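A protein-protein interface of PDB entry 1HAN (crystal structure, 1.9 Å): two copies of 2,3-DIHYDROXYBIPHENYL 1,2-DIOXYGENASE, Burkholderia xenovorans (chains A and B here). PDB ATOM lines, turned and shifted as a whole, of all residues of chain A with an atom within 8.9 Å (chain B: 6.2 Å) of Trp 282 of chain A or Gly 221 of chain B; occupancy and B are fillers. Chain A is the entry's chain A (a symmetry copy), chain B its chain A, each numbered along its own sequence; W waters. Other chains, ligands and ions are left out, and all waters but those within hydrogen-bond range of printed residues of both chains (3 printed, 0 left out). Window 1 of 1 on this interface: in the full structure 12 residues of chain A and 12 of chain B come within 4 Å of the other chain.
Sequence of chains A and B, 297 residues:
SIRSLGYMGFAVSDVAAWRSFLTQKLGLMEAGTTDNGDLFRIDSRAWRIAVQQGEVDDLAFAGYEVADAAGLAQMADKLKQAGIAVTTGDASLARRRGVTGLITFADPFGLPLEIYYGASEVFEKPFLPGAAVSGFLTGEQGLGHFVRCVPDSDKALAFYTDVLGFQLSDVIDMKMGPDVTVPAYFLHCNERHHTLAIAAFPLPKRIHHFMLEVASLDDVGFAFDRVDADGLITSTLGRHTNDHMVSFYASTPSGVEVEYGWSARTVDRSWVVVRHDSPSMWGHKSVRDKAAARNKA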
ATOM      1  N   LEU A 217      30.956  32.407  24.022  1.00  0.00           N
ATOM      2  CA  LEU A 217      29.650  32.402  23.388  1.00  0.00           C
ATOM      3  C   LEU A 217      29.806  32.592  21.875  1.00  0.00           C
ATOM      4  O   LEU A 217      29.123  31.936  21.086  1.00  0.00           O
ATOM      5  CB  LEU A 217      28.764  33.512  23.961  1.00  0.00           C
ATOM      6  CG  LEU A 217      27.400  33.671  23.282  1.00  0.00           C
ATOM      7  CD1 LEU A 217      26.574  32.395  23.414  1.00  0.00           C
ATOM      8  CD2 LEU A 217      26.673  34.829  23.901  1.00  0.00           C
ATOM      9  N   SER A 235      18.592  21.435  16.704  1.00  0.00           N
ATOM     10  CA  SER A 235      18.012  22.072  17.870  1.00  0.00           C
ATOM     11  C   SER A 235      18.632  23.454  18.029  1.00  0.00           C
ATOM     12  O   SER A 235      19.856  23.598  18.027  1.00  0.00           O
ATOM     13  CB  SER A 235      18.294  21.207  19.094  1.00  0.00           C
ATOM     14  OG  SER A 235      17.619  21.690  20.231  1.00  0.00           O
ATOM     15  N   THR A 236      17.780  24.467  18.119  1.00  0.00           N
ATOM     16  CA  THR A 236      18.232  25.842  18.264  1.00  0.00           C
ATOM     17  C   THR A 236      18.995  26.059  19.587  1.00  0.00           C
ATOM     18  O   THR A 236      19.032  25.183  20.455  1.00  0.00           O
ATOM     19  CB  THR A 236      17.032  26.838  18.183  1.00  0.00           C
ATOM     20  OG1 THR A 236      16.163  26.653  19.310  1.00  0.00           O
ATOM     21  CG2 THR A 236      16.226  26.617  16.902  1.00  0.00           C
ATOM     22  N   LEU A 237      19.632  27.220  19.715  1.00  0.00           N
ATOM     23  CA  LEU A 237      20.360  27.561  20.933  1.00  0.00           C
ATOM     24  C   LEU A 237      19.422  27.489  22.131  1.00  0.00           C
ATOM     25  O   LEU A 237      18.259  27.881  22.043  1.00  0.00           O
ATOM     26  CB  LEU A 237      20.924  28.982  20.856  1.00  0.00           C
ATOM     27  CG  LEU A 237      22.269  29.183  20.174  1.00  0.00           C
ATOM     28  CD1 LEU A 237      22.512  30.682  19.993  1.00  0.00           C
ATOM     29  CD2 LEU A 237      23.377  28.535  21.018  1.00  0.00           C
ATOM     30  N   GLY A 238      19.934  26.978  23.238  1.00  0.00           N
ATOM     31  CA  GLY A 238      19.148  26.886  24.448  1.00  0.00           C
ATOM     32  C   GLY A 238      20.074  26.601  25.605  1.00  0.00           C
ATOM     33  O   GLY A 238      21.287  26.454  25.414  1.00  0.00           O
ATOM     34  N   ARG A 239      19.524  26.541  26.810  1.00  0.00           N
ATOM     35  CA  ARG A 239      20.337  26.231  27.970  1.00  0.00           C
ATOM     36  C   ARG A 239      19.700  25.069  28.701  1.00  0.00           C
ATOM     37  O   ARG A 239      18.497  25.089  28.936  1.00  0.00           O
ATOM     38  CB  ARG A 239      20.455  27.415  28.936  1.00  0.00           C
ATOM     39  CG  ARG A 239      21.630  27.178  29.872  1.00  0.00           C
ATOM     40  CD  ARG A 239      21.608  27.960  31.154  1.00  0.00           C
ATOM     41  NE  ARG A 239      22.031  29.342  31.003  1.00  0.00           N
ATOM     42  CZ  ARG A 239      23.272  29.793  31.169  1.00  0.00           C
ATOM     43  NH1 ARG A 239      24.272  28.974  31.484  1.00  0.00           N
ATOM     44  NH2 ARG A 239      23.477  31.097  31.135  1.00  0.00           N
ATOM     45  N   HIS A 240      20.493  24.053  29.037  1.00  0.00           N
ATOM     46  CA  HIS A 240      19.990  22.886  29.764  1.00  0.00           C
ATOM     47  C   HIS A 240      19.756  23.192  31.238  1.00  0.00           C
ATOM     48  O   HIS A 240      20.462  24.010  31.846  1.00  0.00           O
ATOM     49  CB  HIS A 240      20.935  21.692  29.631  1.00  0.00           C
ATOM     50  CG  HIS A 240      20.870  21.033  28.290  1.00  0.00           C
ATOM     51  ND1 HIS A 240      19.711  20.477  27.786  1.00  0.00           N
ATOM     52  CD2 HIS A 240      21.817  20.856  27.338  1.00  0.00           C
ATOM     53  CE1 HIS A 240      19.948  19.983  26.581  1.00  0.00           C
ATOM     54  NE2 HIS A 240      21.219  20.201  26.288  1.00  0.00           N
ATOM     55  N   THR A 241      18.779  22.484  31.805  1.00  0.00           N
ATOM     56  CA  THR A 241      18.374  22.643  33.197  1.00  0.00           C
ATOM     57  C   THR A 241      19.362  22.068  34.191  1.00  0.00           C
ATOM     58  O   THR A 241      19.500  22.581  35.299  1.00  0.00           O
ATOM     59  CB  THR A 241      17.034  21.918  33.469  1.00  0.00           C
ATOM     60  OG1 THR A 241      17.129  20.575  32.974  1.00  0.00           O
ATOM     61  CG2 THR A 241      15.852  22.630  32.810  1.00  0.00           C
ATOM     62  N   HIS A 244      23.453  23.331  32.812  1.00  0.00           N
ATOM     63  CA  HIS A 244      23.391  24.751  32.450  1.00  0.00           C
ATOM     64  C   HIS A 244      24.211  25.123  31.214  1.00  0.00           C
ATOM     65  O   HIS A 244      24.585  26.283  31.016  1.00  0.00           O
ATOM     66  CB  HIS A 244      23.771  25.624  33.648  1.00  0.00           C
ATOM     67  CG  HIS A 244      22.799  25.515  34.775  1.00  0.00           C
ATOM     68  ND1 HIS A 244      22.919  26.226  35.945  1.00  0.00           N
ATOM     69  CD2 HIS A 244      21.682  24.765  34.907  1.00  0.00           C
ATOM     70  CE1 HIS A 244      21.916  25.919  36.751  1.00  0.00           C
ATOM     71  NE2 HIS A 244      21.154  25.034  36.141  1.00  0.00           N
ATOM     72  N   MET A 245      24.458  24.135  30.364  1.00  0.00           N
ATOM     73  CA  MET A 245      25.207  24.340  29.131  1.00  0.00           C
ATOM     74  C   MET A 245      24.342  25.114  28.130  1.00  0.00           C
ATOM     75  O   MET A 245      23.150  24.814  27.970  1.00  0.00           O
ATOM     76  CB  MET A 245      25.554  22.974  28.524  1.00  0.00           C
ATOM     77  CG  MET A 245      26.317  22.999  27.193  1.00  0.00           C
ATOM     78  SD  MET A 245      28.101  22.815  27.402  1.00  0.00           S
ATOM     79  CE  MET A 245      28.176  21.198  28.100  1.00  0.00           C
ATOM     80  N   VAL A 246      24.927  26.133  27.506  1.00  0.00           N
ATOM     81  CA  VAL A 246      24.257  26.909  26.461  1.00  0.00           C
ATOM     82  C   VAL A 246      24.779  26.224  25.200  1.00  0.00           C
ATOM     83  O   VAL A 246      25.988  26.231  24.942  1.00  0.00           O
ATOM     84  CB  VAL A 246      24.685  28.389  26.482  1.00  0.00           C
ATOM     85  CG1 VAL A 246      24.085  29.124  25.278  1.00  0.00           C
ATOM     86  CG2 VAL A 246      24.206  29.047  27.782  1.00  0.00           C
ATOM     87  N   SER A 247      23.889  25.646  24.401  1.00  0.00           N
ATOM     88  CA  SER A 247      24.341  24.896  23.233  1.00  0.00           C
ATOM     89  C   SER A 247      23.309  24.760  22.139  1.00  0.00           C
ATOM     90  O   SER A 247      22.157  25.145  22.311  1.00  0.00           O
ATOM     91  CB  SER A 247      24.664  23.466  23.686  1.00  0.00           C
ATOM     92  OG  SER A 247      23.503  22.820  24.233  1.00  0.00           O
ATOM     93  N   PHE A 248      23.753  24.229  21.006  1.00  0.00           N
ATOM     94  CA  PHE A 248      22.858  23.898  19.901  1.00  0.00           C
ATOM     95  C   PHE A 248      23.256  22.463  19.546  1.00  0.00           C
ATOM     96  O   PHE A 248      24.318  21.981  19.987  1.00  0.00           O
ATOM     97  CB  PHE A 248      22.992  24.854  18.695  1.00  0.00           C
ATOM     98  CG  PHE A 248      24.302  24.747  17.950  1.00  0.00           C
ATOM     99  CD1 PHE A 248      24.488  23.778  16.957  1.00  0.00           C
ATOM    100  CD2 PHE A 248      25.343  25.624  18.228  1.00  0.00           C
ATOM    101  CE1 PHE A 248      25.699  23.683  16.250  1.00  0.00           C
ATOM    102  CE2 PHE A 248      26.555  25.541  17.529  1.00  0.00           C
ATOM    103  CZ  PHE A 248      26.733  24.568  16.537  1.00  0.00           C
ATOM    104  N   TRP A 262      28.729  25.920  25.629  1.00  0.00           N
ATOM    105  CA  TRP A 262      29.548  26.851  26.369  1.00  0.00           C
ATOM    106  C   TRP A 262      28.909  27.153  27.723  1.00  0.00           C
ATOM    107  O   TRP A 262      27.698  27.022  27.893  1.00  0.00           O
ATOM    108  CB  TRP A 262      29.626  28.137  25.529  1.00  0.00           C
ATOM    109  CG  TRP A 262      30.118  29.358  26.232  1.00  0.00           C
ATOM    110  CD1 TRP A 262      31.409  29.638  26.569  1.00  0.00           C
ATOM    111  CD2 TRP A 262      29.324  30.449  26.724  1.00  0.00           C
ATOM    112  NE1 TRP A 262      31.470  30.833  27.246  1.00  0.00           N
ATOM    113  CE2 TRP A 262      30.206  31.351  27.361  1.00  0.00           C
ATOM    114  CE3 TRP A 262      27.951  30.748  26.701  1.00  0.00           C
ATOM    115  CZ2 TRP A 262      29.761  32.535  27.975  1.00  0.00           C
ATOM    116  CZ3 TRP A 262      27.507  31.932  27.316  1.00  0.00           C
ATOM    117  CH2 TRP A 262      28.412  32.803  27.942  1.00  0.00           C
ATOM    118  N   SER A 278      12.103  18.780  32.980  1.00  0.00           N
ATOM    119  CA  SER A 278      12.388  19.363  31.658  1.00  0.00           C
ATOM    120  C   SER A 278      13.888  19.351  31.409  1.00  0.00           C
ATOM    121  O   SER A 278      14.684  19.561  32.335  1.00  0.00           O
ATOM    122  CB  SER A 278      11.943  20.828  31.579  1.00  0.00           C
ATOM    123  OG  SER A 278      10.540  20.961  31.733  1.00  0.00           O
ATOM    124  N   PRO A 279      14.299  19.108  30.157  1.00  0.00           N
ATOM    125  CA  PRO A 279      15.733  19.092  29.858  1.00  0.00           C
ATOM    126  C   PRO A 279      16.307  20.480  29.568  1.00  0.00           C
ATOM    127  O   PRO A 279      17.525  20.659  29.614  1.00  0.00           O
ATOM    128  CB  PRO A 279      15.818  18.175  28.630  1.00  0.00           C
ATOM    129  CG  PRO A 279      14.526  18.470  27.911  1.00  0.00           C
ATOM    130  CD  PRO A 279      13.506  18.552  29.044  1.00  0.00           C
ATOM    131  N   SER A 280      15.457  21.463  29.283  1.00  0.00           N
ATOM    132  CA  SER A 280      15.950  22.798  28.965  1.00  0.00           C
ATOM    133  C   SER A 280      15.204  23.920  29.652  1.00  0.00           C
ATOM    134  O   SER A 280      13.994  23.842  29.821  1.00  0.00           O
ATOM    135  CB  SER A 280      15.897  23.028  27.453  1.00  0.00           C
ATOM    136  OG  SER A 280      16.738  22.110  26.781  1.00  0.00           O
ATOM    137  N   MET A 281      15.944  24.951  30.060  1.00  0.00           N
ATOM    138  CA  MET A 281      15.395  26.157  30.705  1.00  0.00           C
ATOM    139  C   MET A 281      14.730  27.022  29.639  1.00  0.00           C
ATOM    140  O   MET A 281      13.659  27.589  29.864  1.00  0.00           O
ATOM    141  CB  MET A 281      16.510  27.008  31.294  1.00  0.00           C
ATOM    142  CG  MET A 281      17.136  26.492  32.506  1.00  0.00           C
ATOM    143  SD  MET A 281      18.307  27.731  33.053  1.00  0.00           S
ATOM    144  CE  MET A 281      19.472  26.717  33.703  1.00  0.00           C
ATOM    145  N   TRP A 282      15.449  27.220  28.530  1.00  0.00           N
ATOM    146  CA  TRP A 282      14.958  27.992  27.386  1.00  0.00           C
ATOM    147  C   TRP A 282      15.637  27.525  26.107  1.00  0.00           C
ATOM    148  O   TRP A 282      16.671  26.848  26.158  1.00  0.00           O
ATOM    149  CB  TRP A 282      15.164  29.505  27.585  1.00  0.00           C
ATOM    150  CG  TRP A 282      16.561  29.944  27.984  1.00  0.00           C
ATOM    151  CD1 TRP A 282      16.999  30.212  29.249  1.00  0.00           C
ATOM    152  CD2 TRP A 282      17.679  30.205  27.108  1.00  0.00           C
ATOM    153  NE1 TRP A 282      18.309  30.627  29.218  1.00  0.00           N
ATOM    154  CE2 TRP A 282      18.756  30.631  27.926  1.00  0.00           C
ATOM    155  CE3 TRP A 282      17.877  30.128  25.720  1.00  0.00           C
ATOM    156  CZ2 TRP A 282      20.014  30.976  27.403  1.00  0.00           C
ATOM    157  CZ3 TRP A 282      19.139  30.477  25.189  1.00  0.00           C
ATOM    158  CH2 TRP A 282      20.187  30.893  26.036  1.00  0.00           C
ATOM    159  N   GLY A 283      15.014  27.832  24.972  1.00  0.00           N
ATOM    160  CA  GLY A 283      15.566  27.467  23.678  1.00  0.00           C
ATOM    161  C   GLY A 283      15.540  25.982  23.392  1.00  0.00           C
ATOM    162  O   GLY A 283      14.678  25.257  23.895  1.00  0.00           O
ATOM    163  N   HIS A 284      16.508  25.519  22.610  1.00  0.00           N
ATOM    164  CA  HIS A 284      16.584  24.113  22.241  1.00  0.00           C
ATOM    165  C   HIS A 284      15.301  23.645  21.552  1.00  0.00           C
ATOM    166  O   HIS A 284      14.783  22.569  21.822  1.00  0.00           O
ATOM    167  CB  HIS A 284      16.896  23.245  23.452  1.00  0.00           C
ATOM    168  CG  HIS A 284      18.329  23.294  23.875  1.00  0.00           C
ATOM    169  ND1 HIS A 284      18.722  23.153  25.187  1.00  0.00           N
ATOM    170  CD2 HIS A 284      19.466  23.440  23.156  1.00  0.00           C
ATOM    171  CE1 HIS A 284      20.042  23.202  25.258  1.00  0.00           C
ATOM    172  NE2 HIS A 284      20.516  23.373  24.040  1.00  0.00           N
ATOM    173  N   LYS A 285      14.799  24.479  20.656  1.00  0.00           N
ATOM    174  CA  LYS A 285      13.599  24.202  19.886  1.00  0.00           C
ATOM    175  C   LYS A 285      14.014  23.198  18.813  1.00  0.00           C
ATOM    176  O   LYS A 285      14.991  23.411  18.088  1.00  0.00           O
ATOM    177  CB  LYS A 285      13.128  25.511  19.251  1.00  0.00           C
ATOM    178  CG  LYS A 285      11.822  25.486  18.498  1.00  0.00           C
ATOM    179  CD  LYS A 285      11.431  26.923  18.132  1.00  0.00           C
ATOM    180  CE  LYS A 285      10.017  27.045  17.578  1.00  0.00           C
ATOM    181  NZ  LYS A 285       9.616  28.478  17.411  1.00  0.00           N
ATOM    182  N   SER B 216      21.532  39.788  32.104  1.00  0.00           N
ATOM    183  CA  SER B 216      22.135  38.489  31.841  1.00  0.00           C
ATOM    184  C   SER B 216      21.623  37.821  30.575  1.00  0.00           C
ATOM    185  O   SER B 216      20.558  38.183  30.064  1.00  0.00           O
ATOM    186  CB  SER B 216      21.920  37.563  33.033  1.00  0.00           C
ATOM    187  OG  SER B 216      20.642  36.972  32.980  1.00  0.00           O
ATOM    188  N   LEU B 217      22.392  36.852  30.076  1.00  0.00           N
ATOM    189  CA  LEU B 217      22.019  36.098  28.892  1.00  0.00           C
ATOM    190  C   LEU B 217      20.688  35.378  29.132  1.00  0.00           C
ATOM    191  O   LEU B 217      19.827  35.337  28.250  1.00  0.00           O
ATOM    192  CB  LEU B 217      23.104  35.079  28.534  1.00  0.00           C
ATOM    193  CG  LEU B 217      22.762  34.149  27.365  1.00  0.00           C
ATOM    194  CD1 LEU B 217      22.528  34.946  26.086  1.00  0.00           C
ATOM    195  CD2 LEU B 217      23.882  33.168  27.171  1.00  0.00           C
ATOM    196  N   ASP B 218      20.497  34.825  30.323  1.00  0.00           N
ATOM    197  CA  ASP B 218      19.249  34.127  30.611  1.00  0.00           C
ATOM    198  C   ASP B 218      18.023  35.029  30.489  1.00  0.00           C
ATOM    199  O   ASP B 218      16.962  34.571  30.075  1.00  0.00           O
ATOM    200  CB  ASP B 218      19.290  33.466  31.982  1.00  0.00           C
ATOM    201  CG  ASP B 218      20.209  32.266  32.020  1.00  0.00           C
ATOM    202  OD1 ASP B 218      20.357  31.575  31.000  1.00  0.00           O
ATOM    203  OD2 ASP B 218      20.794  32.006  33.087  1.00  0.00           O
ATOM    204  N   ASP B 219      18.170  36.308  30.830  1.00  0.00           N
ATOM    205  CA  ASP B 219      17.054  37.249  30.713  1.00  0.00           C
ATOM    206  C   ASP B 219      16.601  37.256  29.255  1.00  0.00           C
ATOM    207  O   ASP B 219      15.405  37.230  28.955  1.00  0.00           O
ATOM    208  CB  ASP B 219      17.485  38.668  31.097  1.00  0.00           C
ATOM    209  CG  ASP B 219      17.813  38.808  32.568  1.00  0.00           C
ATOM    210  OD1 ASP B 219      17.263  38.052  33.389  1.00  0.00           O
ATOM    211  OD2 ASP B 219      18.620  39.687  32.906  1.00  0.00           O
ATOM    212  N   VAL B 220      17.574  37.286  28.351  1.00  0.00           N
ATOM    213  CA  VAL B 220      17.292  37.284  26.914  1.00  0.00           C
ATOM    214  C   VAL B 220      16.700  35.939  26.472  1.00  0.00           C
ATOM    215  O   VAL B 220      15.721  35.910  25.734  1.00  0.00           O
ATOM    216  CB  VAL B 220      18.581  37.591  26.064  1.00  0.00           C
ATOM    217  CG1 VAL B 220      18.245  37.625  24.576  1.00  0.00           C
ATOM    218  CG2 VAL B 220      19.194  38.914  26.482  1.00  0.00           C
ATOM    219  N   GLY B 221      17.306  34.838  26.913  1.00  0.00           N
ATOM    220  CA  GLY B 221      16.843  33.512  26.552  1.00  0.00           C
ATOM    221  C   GLY B 221      15.426  33.231  27.005  1.00  0.00           C
ATOM    222  O   GLY B 221      14.625  32.701  26.242  1.00  0.00           O
ATOM    223  N   PHE B 222      15.105  33.569  28.250  1.00  0.00           N
ATOM    224  CA  PHE B 222      13.745  33.362  28.748  1.00  0.00           C
ATOM    225  C   PHE B 222      12.735  34.238  28.007  1.00  0.00           C
ATOM    226  O   PHE B 222      11.654  33.767  27.642  1.00  0.00           O
ATOM    227  CB  PHE B 222      13.673  33.643  30.253  1.00  0.00           C
ATOM    228  CG  PHE B 222      14.182  32.513  31.106  1.00  0.00           C
ATOM    229  CD1 PHE B 222      13.575  31.264  31.047  1.00  0.00           C
ATOM    230  CD2 PHE B 222      15.246  32.702  31.983  1.00  0.00           C
ATOM    231  CE1 PHE B 222      14.016  30.223  31.846  1.00  0.00           C
ATOM    232  CE2 PHE B 222      15.699  31.653  32.794  1.00  0.00           C
ATOM    233  CZ  PHE B 222      15.080  30.418  32.721  1.00  0.00           C
ATOM    234  N   ALA B 223      13.074  35.510  27.791  1.00  0.00           N
ATOM    235  CA  ALA B 223      12.179  36.423  27.086  1.00  0.00           C
ATOM    236  C   ALA B 223      11.919  35.944  25.658  1.00  0.00           C
ATOM    237  O   ALA B 223      10.806  36.081  25.148  1.00  0.00           O
ATOM    238  CB  ALA B 223      12.747  37.846  27.076  1.00  0.00           C
ATOM    239  N   PHE B 224      12.947  35.402  25.011  1.00  0.00           N
ATOM    240  CA  PHE B 224      12.812  34.905  23.643  1.00  0.00           C
ATOM    241  C   PHE B 224      11.695  33.862  23.578  1.00  0.00           C
ATOM    242  O   PHE B 224      10.817  33.940  22.716  1.00  0.00           O
ATOM    243  CB  PHE B 224      14.142  34.306  23.150  1.00  0.00           C
ATOM    244  CG  PHE B 224      14.108  33.866  21.716  1.00  0.00           C
ATOM    245  CD1 PHE B 224      13.480  32.672  21.352  1.00  0.00           C
ATOM    246  CD2 PHE B 224      14.674  34.657  20.723  1.00  0.00           C
ATOM    247  CE1 PHE B 224      13.421  32.280  20.018  1.00  0.00           C
ATOM    248  CE2 PHE B 224      14.617  34.270  19.384  1.00  0.00           C
ATOM    249  CZ  PHE B 224      13.990  33.081  19.036  1.00  0.00           C
ATOM    250  N   ASP B 225      11.718  32.902  24.498  1.00  0.00           N
ATOM    251  CA  ASP B 225      10.698  31.855  24.529  1.00  0.00           C
ATOM    252  C   ASP B 225       9.313  32.418  24.807  1.00  0.00           C
ATOM    253  O   ASP B 225       8.334  31.943  24.238  1.00  0.00           O
ATOM    254  CB  ASP B 225      11.045  30.787  25.567  1.00  0.00           C
ATOM    255  CG  ASP B 225      12.092  29.805  25.070  1.00  0.00           C
ATOM    256  OD1 ASP B 225      12.615  29.989  23.962  1.00  0.00           O
ATOM    257  OD2 ASP B 225      12.386  28.833  25.783  1.00  0.00           O
ATOM    258  N   ARG B 226       9.216  33.414  25.689  1.00  0.00           N
ATOM    259  CA  ARG B 226       7.925  34.032  26.011  1.00  0.00           C
ATOM    260  C   ARG B 226       7.301  34.677  24.779  1.00  0.00           C
ATOM    261  O   ARG B 226       6.092  34.550  24.526  1.00  0.00           O
ATOM    262  CB  ARG B 226       8.075  35.086  27.116  1.00  0.00           C
ATOM    263  CG  ARG B 226       8.440  34.495  28.463  1.00  0.00           C
ATOM    264  CD  ARG B 226       8.188  35.463  29.602  1.00  0.00           C
ATOM    265  NE  ARG B 226       8.991  36.674  29.500  1.00  0.00           N
ATOM    266  CZ  ARG B 226      10.162  36.852  30.103  1.00  0.00           C
ATOM    267  NH1 ARG B 226      10.691  35.888  30.848  1.00  0.00           N
ATOM    268  NH2 ARG B 226      10.788  38.011  29.983  1.00  0.00           N
ATOM    269  N   LEU B 237      18.292  35.073  17.677  1.00  0.00           N
ATOM    270  CA  LEU B 237      19.416  35.568  18.466  1.00  0.00           C
ATOM    271  C   LEU B 237      20.630  35.764  17.565  1.00  0.00           C
ATOM    272  O   LEU B 237      20.883  34.961  16.668  1.00  0.00           O
ATOM    273  CB  LEU B 237      19.796  34.574  19.565  1.00  0.00           C
ATOM    274  CG  LEU B 237      19.038  34.638  20.882  1.00  0.00           C
ATOM    275  CD1 LEU B 237      19.404  33.414  21.724  1.00  0.00           C
ATOM    276  CD2 LEU B 237      19.385  35.942  21.614  1.00  0.00           C
ATOM    277  N   PHE B 248      17.678  39.648  20.184  1.00  0.00           N
ATOM    278  CA  PHE B 248      16.688  39.127  19.248  1.00  0.00           C
ATOM    279  C   PHE B 248      15.755  40.321  19.024  1.00  0.00           C
ATOM    280  O   PHE B 248      15.806  41.305  19.788  1.00  0.00           O
ATOM    281  CB  PHE B 248      15.931  37.890  19.778  1.00  0.00           C
ATOM    282  CG  PHE B 248      15.003  38.169  20.938  1.00  0.00           C
ATOM    283  CD1 PHE B 248      13.701  38.634  20.721  1.00  0.00           C
ATOM    284  CD2 PHE B 248      15.424  37.953  22.244  1.00  0.00           C
ATOM    285  CE1 PHE B 248      12.828  38.882  21.795  1.00  0.00           C
ATOM    286  CE2 PHE B 248      14.564  38.194  23.323  1.00  0.00           C
ATOM    287  CZ  PHE B 248      13.262  38.660  23.098  1.00  0.00           C
HETATM  288  O   HOH W   1      15.174  31.041  23.835  1.00  0.00           O
HETATM  289  O   HOH W   2      22.811  34.084  32.600  1.00  0.00           O
HETATM  290  O   HOH W   3      11.571  29.095  28.606  1.00  0.00           O
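Among the printed residues, pairs that only touch across the chains: Trp 262 of chain A with Leu 217 of chain B, Met 281 of chain A with Phe 222 of chain B, Trp 282 of chain A with Gly 221 of chain B, Trp 282 of chain A with Phe 222 of chain B and Trp 282 of chain A with Asp 225 of chain B.
The backbone NH of Asp 218 of chain B lies close to the side-chain hydroxyl of Ser 216 of chain B (3.4 Å).
The backbone carbonyl oxygen (O) of His 244 of chain A sits at hydrogen-bond distance from the guanidinium group (NH1) of Arg 239 of chain A, 2.7 Å away.
The backbone NH (N) of Met 281 of chain A sits at hydrogen-bond distance from the backbone carbonyl oxygen (O) of Arg 239 of chain A, at 2.8 Å.
O of Trp 282 of chain A lies within hydrogen-bond range of N of Arg 239 of chain A (2.9 Å).
The side-chain sulfur (SD) of Met 245 of chain A sits at hydrogen-bond distance from the backbone NH (N) of Trp 262 of chain A (3.6 Å).
The backbone carbonyl oxygen (O) of Val 246 of chain A lies within hydrogen-bond range of the backbone NH (N) of Trp 262 of chain A, 2.8 Å away.
Hydrophobic or aromatic side chains of chain A that line the printed part of chain B: Trp 262, Met 281 and Trp 282.
Of the 13 printed residues of chain B, 5 touch a printed residue of chain A.
Hydrophobic or aromatic side chains of chain B within 4 Å of the printed part of chain A: Leu 217 and Phe 222.
Among the printed residues, Asp or Glu carboxylates within 4 Å of a Lys or Arg side-chain nitrogen of the other chain: Arg 239 of chain A with Asp 218 of chain B.
Positions printed for both chains: 217, 237 and 248.
Trp 282 of chain A touches just these residues of chain B: Asp 218 (2.9 Å), Gly 221 (3.5 Å), Phe 222 (3.9 Å) and Asp 225 (3.1 Å).
Of chain A, only Trp 282 (3.5 Å) comes within 4 Å of Gly 221 of chain B.
Of chain A, only Arg 239 and Trp 282 come within 4 Å of Asp 218 of chain B.
No residue of chain A comes within 4 Å of Val 220 of chain B.
Printed residues of chain B within 4 Å of Arg 239 of chain A: Asp 218 (2.8 Å).
Of the printed residues of chain A, Leu 217 of chain B touches Trp 262.
Of the printed residues of chain B, Trp 262 of chain A touches Leu 217 (3.8 Å).
Of the printed residues of chain B, Gly 283 of chain A touches Asp 225.
Arg 226 of chain B touches none of the printed residues of chain A.
Ser 216 of chain B touches none of the printed residues of chain A.
The nearest residue of chain A that does not touch Gly 221 of chain B is Gly 283 of chain A (5.0 Å).
Water W1 lies within hydrogen-bond range of OD1 of Asp 225 of chain B (2.8 Å), O of Gly 221 of chain B (3.0 Å) and N of Gly 283 of chain A (3.4 Å).
Water W3 bridges O of Met 281 of chain A (2.9 Å) and OD2 of Asp 225 of chain B (2.9 Å).
Water W2 bridges the side-chain carboxylate (OD2) of Asp 218 of chain B (2.9 Å) and the guanidinium group (NH2) of Arg 239 of chain A (3.4 Å).
The side-chain carboxylate of Asp 218 of chain B is in salt-bridge range of the guanidinium group of Arg 239 of chain A (2.8 Å).
The side-chain carboxylate (OD1) of Asp 218 of chain B sits at hydrogen-bond distance from the indole nitrogen (NE1) of Trp 282 of chain A (2.9 Å).
The side-chain carboxylate (OD2) of Asp 225 of chain B sits at hydrogen-bond distance from the backbone NH (N) of Gly 283 of chain A (2.9 Å).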
